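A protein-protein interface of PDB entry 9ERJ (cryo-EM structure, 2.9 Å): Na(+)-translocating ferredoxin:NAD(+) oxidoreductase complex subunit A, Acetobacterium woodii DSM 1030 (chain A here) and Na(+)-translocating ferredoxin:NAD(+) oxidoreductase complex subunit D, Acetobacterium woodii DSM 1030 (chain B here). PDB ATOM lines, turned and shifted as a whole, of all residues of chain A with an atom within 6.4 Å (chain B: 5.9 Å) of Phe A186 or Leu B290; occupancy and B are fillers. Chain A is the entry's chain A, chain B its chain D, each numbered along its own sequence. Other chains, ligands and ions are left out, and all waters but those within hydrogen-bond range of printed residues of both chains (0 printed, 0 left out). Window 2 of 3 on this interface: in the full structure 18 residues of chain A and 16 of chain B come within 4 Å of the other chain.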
ATOM      1  N   PHE A  12      23.759  22.588 -18.402  1.00  0.00           N
ATOM      2  CA  PHE A  12      22.628  22.671 -17.481  1.00  0.00           C
ATOM      3  C   PHE A  12      22.240  24.107 -17.136  1.00  0.00           C
ATOM      4  O   PHE A  12      21.089  24.508 -17.334  1.00  0.00           O
ATOM      5  CB  PHE A  12      22.945  21.890 -16.201  1.00  0.00           C
ATOM      6  CG  PHE A  12      22.925  20.401 -16.380  1.00  0.00           C
ATOM      7  CD1 PHE A  12      21.744  19.740 -16.665  1.00  0.00           C
ATOM      8  CD2 PHE A  12      24.091  19.662 -16.267  1.00  0.00           C
ATOM      9  CE1 PHE A  12      21.723  18.371 -16.833  1.00  0.00           C
ATOM     10  CE2 PHE A  12      24.076  18.291 -16.433  1.00  0.00           C
ATOM     11  CZ  PHE A  12      22.890  17.645 -16.717  1.00  0.00           C
ATOM     12  N   VAL A  13      23.186  24.885 -16.604  1.00  0.00           N
ATOM     13  CA  VAL A  13      22.855  26.198 -16.054  1.00  0.00           C
ATOM     14  C   VAL A  13      22.465  27.176 -17.157  1.00  0.00           C
ATOM     15  O   VAL A  13      21.560  28.000 -16.982  1.00  0.00           O
ATOM     16  CB  VAL A  13      24.027  26.731 -15.211  1.00  0.00           C
ATOM     17  CG1 VAL A  13      23.582  27.919 -14.375  1.00  0.00           C
ATOM     18  CG2 VAL A  13      24.582  25.630 -14.322  1.00  0.00           C
ATOM     19  N   ASN A  14      23.131  27.104 -18.306  1.00  0.00           N
ATOM     20  CA  ASN A  14      22.958  28.065 -19.392  1.00  0.00           C
ATOM     21  C   ASN A  14      22.638  27.349 -20.699  1.00  0.00           C
ATOM     22  O   ASN A  14      23.305  27.540 -21.718  1.00  0.00           O
ATOM     23  CB  ASN A  14      24.191  28.949 -19.542  1.00  0.00           C
ATOM     24  CG  ASN A  14      24.005  30.318 -18.913  1.00  0.00           C
ATOM     25  OD1 ASN A  14      23.050  31.030 -19.221  1.00  0.00           O
ATOM     26  ND2 ASN A  14      24.922  30.691 -18.027  1.00  0.00           N
ATOM     27  N   SER A  19      17.206  28.874 -22.411  1.00  0.00           N
ATOM     28  CA  SER A  19      17.605  30.126 -21.771  1.00  0.00           C
ATOM     29  C   SER A  19      17.955  31.205 -22.792  1.00  0.00           C
ATOM     30  O   SER A  19      17.397  32.307 -22.760  1.00  0.00           O
ATOM     31  CB  SER A  19      18.784  29.881 -20.827  1.00  0.00           C
ATOM     32  OG  SER A  19      18.472  28.884 -19.871  1.00  0.00           O
ATOM     33  N   MET A 179       8.695  23.534 -19.761  1.00  0.00           N
ATOM     34  CA  MET A 179      10.076  23.070 -19.631  1.00  0.00           C
ATOM     35  C   MET A 179      11.023  24.212 -19.283  1.00  0.00           C
ATOM     36  O   MET A 179      11.993  24.012 -18.541  1.00  0.00           O
ATOM     37  CB  MET A 179      10.533  22.383 -20.917  1.00  0.00           C
ATOM     38  CG  MET A 179       9.700  21.186 -21.328  1.00  0.00           C
ATOM     39  SD  MET A 179      10.205  20.506 -22.918  1.00  0.00           S
ATOM     40  CE  MET A 179      11.924  20.131 -22.597  1.00  0.00           C
ATOM     41  N   ILE A 181      10.267  26.802 -17.410  1.00  0.00           N
ATOM     42  CA  ILE A 181      10.139  27.000 -15.964  1.00  0.00           C
ATOM     43  C   ILE A 181      10.927  25.935 -15.200  1.00  0.00           C
ATOM     44  O   ILE A 181      11.694  26.242 -14.267  1.00  0.00           O
ATOM     45  CB  ILE A 181       8.655  27.001 -15.551  1.00  0.00           C
ATOM     46  CG1 ILE A 181       7.905  28.146 -16.232  1.00  0.00           C
ATOM     47  CG2 ILE A 181       8.522  27.094 -14.040  1.00  0.00           C
ATOM     48  CD1 ILE A 181       6.478  28.310 -15.757  1.00  0.00           C
ATOM     49  N   ALA A 182      10.761  24.667 -15.596  1.00  0.00           N
ATOM     50  CA  ALA A 182      11.450  23.573 -14.914  1.00  0.00           C
ATOM     51  C   ALA A 182      12.964  23.752 -14.960  1.00  0.00           C
ATOM     52  O   ALA A 182      13.676  23.362 -14.028  1.00  0.00           O
ATOM     53  CB  ALA A 182      11.045  22.233 -15.528  1.00  0.00           C
ATOM     54  N   PHE A 183      13.476  24.350 -16.041  1.00  0.00           N
ATOM     55  CA  PHE A 183      14.900  24.661 -16.114  1.00  0.00           C
ATOM     56  C   PHE A 183      15.253  26.002 -15.478  1.00  0.00           C
ATOM     57  O   PHE A 183      16.426  26.228 -15.161  1.00  0.00           O
ATOM     58  CB  PHE A 183      15.374  24.631 -17.566  1.00  0.00           C
ATOM     59  CG  PHE A 183      16.026  23.338 -17.958  1.00  0.00           C
ATOM     60  CD1 PHE A 183      15.265  22.210 -18.205  1.00  0.00           C
ATOM     61  CD2 PHE A 183      17.403  23.248 -18.067  1.00  0.00           C
ATOM     62  CE1 PHE A 183      15.863  21.018 -18.563  1.00  0.00           C
ATOM     63  CE2 PHE A 183      18.007  22.059 -18.424  1.00  0.00           C
ATOM     64  CZ  PHE A 183      17.236  20.944 -18.672  1.00  0.00           C
ATOM     65  N   LEU A 184      14.274  26.894 -15.284  1.00  0.00           N
ATOM     66  CA  LEU A 184      14.480  28.055 -14.421  1.00  0.00           C
ATOM     67  C   LEU A 184      14.738  27.627 -12.991  1.00  0.00           C
ATOM     68  O   LEU A 184      15.260  28.411 -12.191  1.00  0.00           O
ATOM     69  CB  LEU A 184      13.271  28.991 -14.459  1.00  0.00           C
ATOM     70  CG  LEU A 184      13.399  30.368 -15.106  1.00  0.00           C
ATOM     71  CD1 LEU A 184      12.159  31.186 -14.803  1.00  0.00           C
ATOM     72  CD2 LEU A 184      14.641  31.083 -14.612  1.00  0.00           C
ATOM     73  N   GLY A 185      14.347  26.399 -12.647  1.00  0.00           N
ATOM     74  CA  GLY A 185      14.823  25.814 -11.401  1.00  0.00           C
ATOM     75  C   GLY A 185      16.338  25.780 -11.290  1.00  0.00           C
ATOM     76  O   GLY A 185      16.891  25.861 -10.190  1.00  0.00           O
ATOM     77  N   PHE A 186      17.032  25.653 -12.424  1.00  0.00           N
ATOM     78  CA  PHE A 186      18.498  25.615 -12.472  1.00  0.00           C
ATOM     79  C   PHE A 186      19.035  27.034 -12.648  1.00  0.00           C
ATOM     80  O   PHE A 186      19.417  27.460 -13.741  1.00  0.00           O
ATOM     81  CB  PHE A 186      18.973  24.712 -13.604  1.00  0.00           C
ATOM     82  CG  PHE A 186      19.447  23.366 -13.154  1.00  0.00           C
ATOM     83  CD1 PHE A 186      20.436  23.250 -12.196  1.00  0.00           C
ATOM     84  CD2 PHE A 186      18.908  22.214 -13.697  1.00  0.00           C
ATOM     85  CE1 PHE A 186      20.875  22.009 -11.782  1.00  0.00           C
ATOM     86  CE2 PHE A 186      19.342  20.972 -13.289  1.00  0.00           C
ATOM     87  CZ  PHE A 186      20.326  20.868 -12.330  1.00  0.00           C
ATOM     88  N   SER A 187      19.069  27.781 -11.548  1.00  0.00           N
ATOM     89  CA  SER A 187      19.492  29.173 -11.616  1.00  0.00           C
ATOM     90  C   SER A 187      20.206  29.555 -10.330  1.00  0.00           C
ATOM     91  O   SER A 187      19.966  28.976  -9.267  1.00  0.00           O
ATOM     92  CB  SER A 187      18.303  30.107 -11.866  1.00  0.00           C
ATOM     93  OG  SER A 187      18.628  31.443 -11.532  1.00  0.00           O
ATOM     94  N   GLY A 188      21.089  30.544 -10.445  1.00  0.00           N
ATOM     95  CA  GLY A 188      21.828  31.059  -9.313  1.00  0.00           C
ATOM     96  C   GLY A 188      23.027  30.239  -8.893  1.00  0.00           C
ATOM     97  O   GLY A 188      23.677  30.590  -7.901  1.00  0.00           O
ATOM     98  N   MET A 189      23.343  29.165  -9.610  1.00  0.00           N
ATOM     99  CA  MET A 189      24.446  28.294  -9.230  1.00  0.00           C
ATOM    100  C   MET A 189      25.776  28.924  -9.623  1.00  0.00           C
ATOM    101  O   MET A 189      26.000  29.246 -10.794  1.00  0.00           O
ATOM    102  CB  MET A 189      24.295  26.925  -9.891  1.00  0.00           C
ATOM    103  CG  MET A 189      23.622  25.891  -9.010  1.00  0.00           C
ATOM    104  SD  MET A 189      24.063  24.200  -9.439  1.00  0.00           S
ATOM    105  CE  MET A 189      22.601  23.330  -8.884  1.00  0.00           C
ATOM    106  N   ILE B 270      18.509  15.576  -6.979  1.00  0.00           N
ATOM    107  CA  ILE B 270      18.423  16.975  -7.395  1.00  0.00           C
ATOM    108  C   ILE B 270      17.999  17.889  -6.249  1.00  0.00           C
ATOM    109  O   ILE B 270      18.384  19.064  -6.232  1.00  0.00           O
ATOM    110  CB  ILE B 270      17.477  17.128  -8.602  1.00  0.00           C
ATOM    111  CG1 ILE B 270      17.828  16.110  -9.685  1.00  0.00           C
ATOM    112  CG2 ILE B 270      17.565  18.522  -9.200  1.00  0.00           C
ATOM    113  CD1 ILE B 270      16.953  16.201 -10.914  1.00  0.00           C
ATOM    114  N   ILE B 273      21.243  18.490  -4.308  1.00  0.00           N
ATOM    115  CA  ILE B 273      22.166  19.293  -5.103  1.00  0.00           C
ATOM    116  C   ILE B 273      21.829  20.783  -5.015  1.00  0.00           C
ATOM    117  O   ILE B 273      22.722  21.605  -4.789  1.00  0.00           O
ATOM    118  CB  ILE B 273      22.192  18.812  -6.565  1.00  0.00           C
ATOM    119  CG1 ILE B 273      22.946  17.486  -6.676  1.00  0.00           C
ATOM    120  CG2 ILE B 273      22.841  19.846  -7.468  1.00  0.00           C
ATOM    121  CD1 ILE B 273      22.813  16.824  -8.026  1.00  0.00           C
ATOM    122  N   ILE B 274      20.552  21.149  -5.171  1.00  0.00           N
ATOM    123  CA  ILE B 274      20.131  22.543  -5.025  1.00  0.00           C
ATOM    124  C   ILE B 274      20.220  23.042  -3.592  1.00  0.00           C
ATOM    125  O   ILE B 274      20.581  24.206  -3.375  1.00  0.00           O
ATOM    126  CB  ILE B 274      18.696  22.733  -5.557  1.00  0.00           C
ATOM    127  CG1 ILE B 274      18.579  22.187  -6.979  1.00  0.00           C
ATOM    128  CG2 ILE B 274      18.295  24.198  -5.545  1.00  0.00           C
ATOM    129  CD1 ILE B 274      17.188  22.290  -7.557  1.00  0.00           C
ATOM    130  N   TYR B 280      18.907  28.573  -3.804  1.00  0.00           N
ATOM    131  CA  TYR B 280      17.661  28.487  -3.058  1.00  0.00           C
ATOM    132  C   TYR B 280      17.924  27.770  -1.744  1.00  0.00           C
ATOM    133  O   TYR B 280      18.808  26.908  -1.671  1.00  0.00           O
ATOM    134  CB  TYR B 280      16.578  27.722  -3.836  1.00  0.00           C
ATOM    135  CG  TYR B 280      16.168  28.347  -5.149  1.00  0.00           C
ATOM    136  CD1 TYR B 280      15.198  29.339  -5.196  1.00  0.00           C
ATOM    137  CD2 TYR B 280      16.733  27.929  -6.345  1.00  0.00           C
ATOM    138  CE1 TYR B 280      14.815  29.906  -6.395  1.00  0.00           C
ATOM    139  CE2 TYR B 280      16.356  28.490  -7.547  1.00  0.00           C
ATOM    140  CZ  TYR B 280      15.398  29.476  -7.567  1.00  0.00           C
ATOM    141  OH  TYR B 280      15.021  30.035  -8.764  1.00  0.00           O
ATOM    142  N   SER B 285      10.638  21.490  -5.013  1.00  0.00           N
ATOM    143  CA  SER B 285       9.667  21.747  -6.074  1.00  0.00           C
ATOM    144  C   SER B 285      10.285  21.558  -7.453  1.00  0.00           C
ATOM    145  O   SER B 285       9.710  20.885  -8.316  1.00  0.00           O
ATOM    146  CB  SER B 285       9.107  23.162  -5.925  1.00  0.00           C
ATOM    147  OG  SER B 285       8.508  23.605  -7.129  1.00  0.00           O
ATOM    148  N   TYR B 286      11.467  22.128  -7.673  1.00  0.00           N
ATOM    149  CA  TYR B 286      12.119  22.008  -8.969  1.00  0.00           C
ATOM    150  C   TYR B 286      12.698  20.622  -9.208  1.00  0.00           C
ATOM    151  O   TYR B 286      12.769  20.190 -10.363  1.00  0.00           O
ATOM    152  CB  TYR B 286      13.211  23.068  -9.108  1.00  0.00           C
ATOM    153  CG  TYR B 286      12.705  24.477  -8.902  1.00  0.00           C
ATOM    154  CD1 TYR B 286      11.854  25.069  -9.824  1.00  0.00           C
ATOM    155  CD2 TYR B 286      13.078  25.215  -7.788  1.00  0.00           C
ATOM    156  CE1 TYR B 286      11.390  26.355  -9.646  1.00  0.00           C
ATOM    157  CE2 TYR B 286      12.617  26.501  -7.600  1.00  0.00           C
ATOM    158  CZ  TYR B 286      11.773  27.066  -8.532  1.00  0.00           C
ATOM    159  OH  TYR B 286      11.310  28.348  -8.352  1.00  0.00           O
ATOM    160  N   SER B 287      13.107  19.916  -8.151  1.00  0.00           N
ATOM    161  CA  SER B 287      13.537  18.530  -8.315  1.00  0.00           C
ATOM    162  C   SER B 287      12.381  17.644  -8.758  1.00  0.00           C
ATOM    163  O   SER B 287      12.556  16.772  -9.615  1.00  0.00           O
ATOM    164  CB  SER B 287      14.142  18.003  -7.017  1.00  0.00           C
ATOM    165  OG  SER B 287      13.136  17.743  -6.057  1.00  0.00           O
ATOM    166  N   ILE B 288      11.193  17.846  -8.182  1.00  0.00           N
ATOM    167  CA  ILE B 288      10.025  17.102  -8.641  1.00  0.00           C
ATOM    168  C   ILE B 288       9.603  17.514 -10.047  1.00  0.00           C
ATOM    169  O   ILE B 288       9.291  16.644 -10.869  1.00  0.00           O
ATOM    170  CB  ILE B 288       8.852  17.262  -7.657  1.00  0.00           C
ATOM    171  CG1 ILE B 288       9.205  16.641  -6.304  1.00  0.00           C
ATOM    172  CG2 ILE B 288       7.592  16.613  -8.197  1.00  0.00           C
ATOM    173  CD1 ILE B 288       8.272  17.046  -5.191  1.00  0.00           C
ATOM    174  N   LEU B 289       9.607  18.811 -10.359  1.00  0.00           N
ATOM    175  CA  LEU B 289       9.226  19.291 -11.682  1.00  0.00           C
ATOM    176  C   LEU B 289      10.186  18.863 -12.784  1.00  0.00           C
ATOM    177  O   LEU B 289       9.754  18.700 -13.928  1.00  0.00           O
ATOM    178  CB  LEU B 289       9.124  20.820 -11.687  1.00  0.00           C
ATOM    179  CG  LEU B 289       7.885  21.468 -11.071  1.00  0.00           C
ATOM    180  CD1 LEU B 289       8.033  22.978 -11.076  1.00  0.00           C
ATOM    181  CD2 LEU B 289       6.634  21.049 -11.815  1.00  0.00           C
ATOM    182  N   LEU B 290      11.471  18.682 -12.478  1.00  0.00           N
ATOM    183  CA  LEU B 290      12.446  18.255 -13.470  1.00  0.00           C
ATOM    184  C   LEU B 290      12.375  16.765 -13.771  1.00  0.00           C
ATOM    185  O   LEU B 290      12.880  16.338 -14.814  1.00  0.00           O
ATOM    186  CB  LEU B 290      13.863  18.613 -13.009  1.00  0.00           C
ATOM    187  CG  LEU B 290      14.420  19.951 -13.497  1.00  0.00           C
ATOM    188  CD1 LEU B 290      15.490  20.468 -12.550  1.00  0.00           C
ATOM    189  CD2 LEU B 290      14.968  19.821 -14.904  1.00  0.00           C
ATOM    190  N   MET B 291      11.767  15.969 -12.891  1.00  0.00           N
ATOM    191  CA  MET B 291      11.575  14.544 -13.124  1.00  0.00           C
ATOM    192  C   MET B 291      10.226  14.236 -13.758  1.00  0.00           C
ATOM    193  O   MET B 291       9.976  13.087 -14.134  1.00  0.00           O
ATOM    194  CB  MET B 291      11.734  13.768 -11.817  1.00  0.00           C
ATOM    195  CG  MET B 291      13.167  13.672 -11.330  1.00  0.00           C
ATOM    196  SD  MET B 291      14.041  12.268 -12.044  1.00  0.00           S
ATOM    197  CE  MET B 291      15.345  13.100 -12.940  1.00  0.00           C
ATOM    198  N   ASN B 292       9.349  15.233 -13.880  1.00  0.00           N
ATOM    199  CA  ASN B 292       8.144  15.112 -14.689  1.00  0.00           C
ATOM    200  C   ASN B 292       8.435  15.244 -16.175  1.00  0.00           C
ATOM    201  O   ASN B 292       7.628  14.795 -16.994  1.00  0.00           O
ATOM    202  CB  ASN B 292       7.120  16.175 -14.278  1.00  0.00           C
ATOM    203  CG  ASN B 292       6.523  15.912 -12.917  1.00  0.00           C
ATOM    204  OD1 ASN B 292       6.723  14.849 -12.334  1.00  0.00           O
ATOM    205  ND2 ASN B 292       5.789  16.884 -12.396  1.00  0.00           N
ATOM    206  N   VAL B 293       9.567  15.847 -16.531  1.00  0.00           N
ATOM    207  CA  VAL B 293       9.993  15.964 -17.920  1.00  0.00           C
ATOM    208  C   VAL B 293      10.682  14.698 -18.419  1.00  0.00           C
ATOM    209  O   VAL B 293      10.446  14.289 -19.566  1.00  0.00           O
ATOM    210  CB  VAL B 293      10.916  17.191 -18.087  1.00  0.00           C
ATOM    211  CG1 VAL B 293      11.471  17.281 -19.495  1.00  0.00           C
ATOM    212  CG2 VAL B 293      10.173  18.467 -17.724  1.00  0.00           C
ATOM    213  N   ALA B 294      11.496  14.049 -17.588  1.00  0.00           N
ATOM    214  CA  ALA B 294      12.232  12.854 -17.972  1.00  0.00           C
ATOM    215  C   ALA B 294      11.413  11.578 -17.827  1.00  0.00           C
ATOM    216  O   ALA B 294      11.908  10.499 -18.165  1.00  0.00           O
ATOM    217  CB  ALA B 294      13.515  12.742 -17.149  1.00  0.00           C
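Among the printed residues, pairs that only touch across the chains: Gly A185 with Tyr B286 (3.4 Å), Ala A182 with Leu B290 (3.5 Å), Gly A185 with Tyr B280 (3.8 Å), Met A189 with Ile B273 (3.8 Å), Leu A184 with Tyr B280 (3.8 Å), Phe A183 with Leu B290 (3.95 Å) and Phe A186 with Leu B290 (3.95 Å).
Printed residues of chain B that touch a printed residue of chain A: Ile B273, Tyr B280, Tyr B286 and Leu B290. Hydrophobic or aromatic side chains of chain B that line the printed part of chain A: Ile B273, Tyr B280, Tyr B286 and Leu B290. Of the 14 printed residues of chain A, 6 touch a printed residue of chain B. Printed residues of chain A that touch a printed residue of chain B: Ala A182, Phe A183, Leu A184, Gly A185, Phe A186 and Met A189. Hydrophobic or aromatic side chains of chain A that line the printed part of chain B: Phe A183, Phe A186 and Met A189. Among the printed residues, no Asp or Glu carboxylate lies within 4 Å of a Lys or Arg side-chain nitrogen of the other chain.
Phe A186 touches just one residue of chain B: Leu B290. Of chain A, only Ala A182, Phe A183 and Phe A186 come within 4 Å of Leu B290. Printed residues of chain A within 4 Å of Tyr B280: Leu A184 (3.8 Å) and Gly A185 (3.8 Å). Of the printed residues of chain A, Tyr B286 touches Gly A185. The nearest residue of chain B that does not touch Phe A186 is Ile B270 (4.8 Å). The nearest residue of chain A that does not touch Leu B290 is Gly A185 (5.5 Å). The nearest printed residue of chain A that does not touch Tyr B280 is Ser A187 (4.03 Å).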
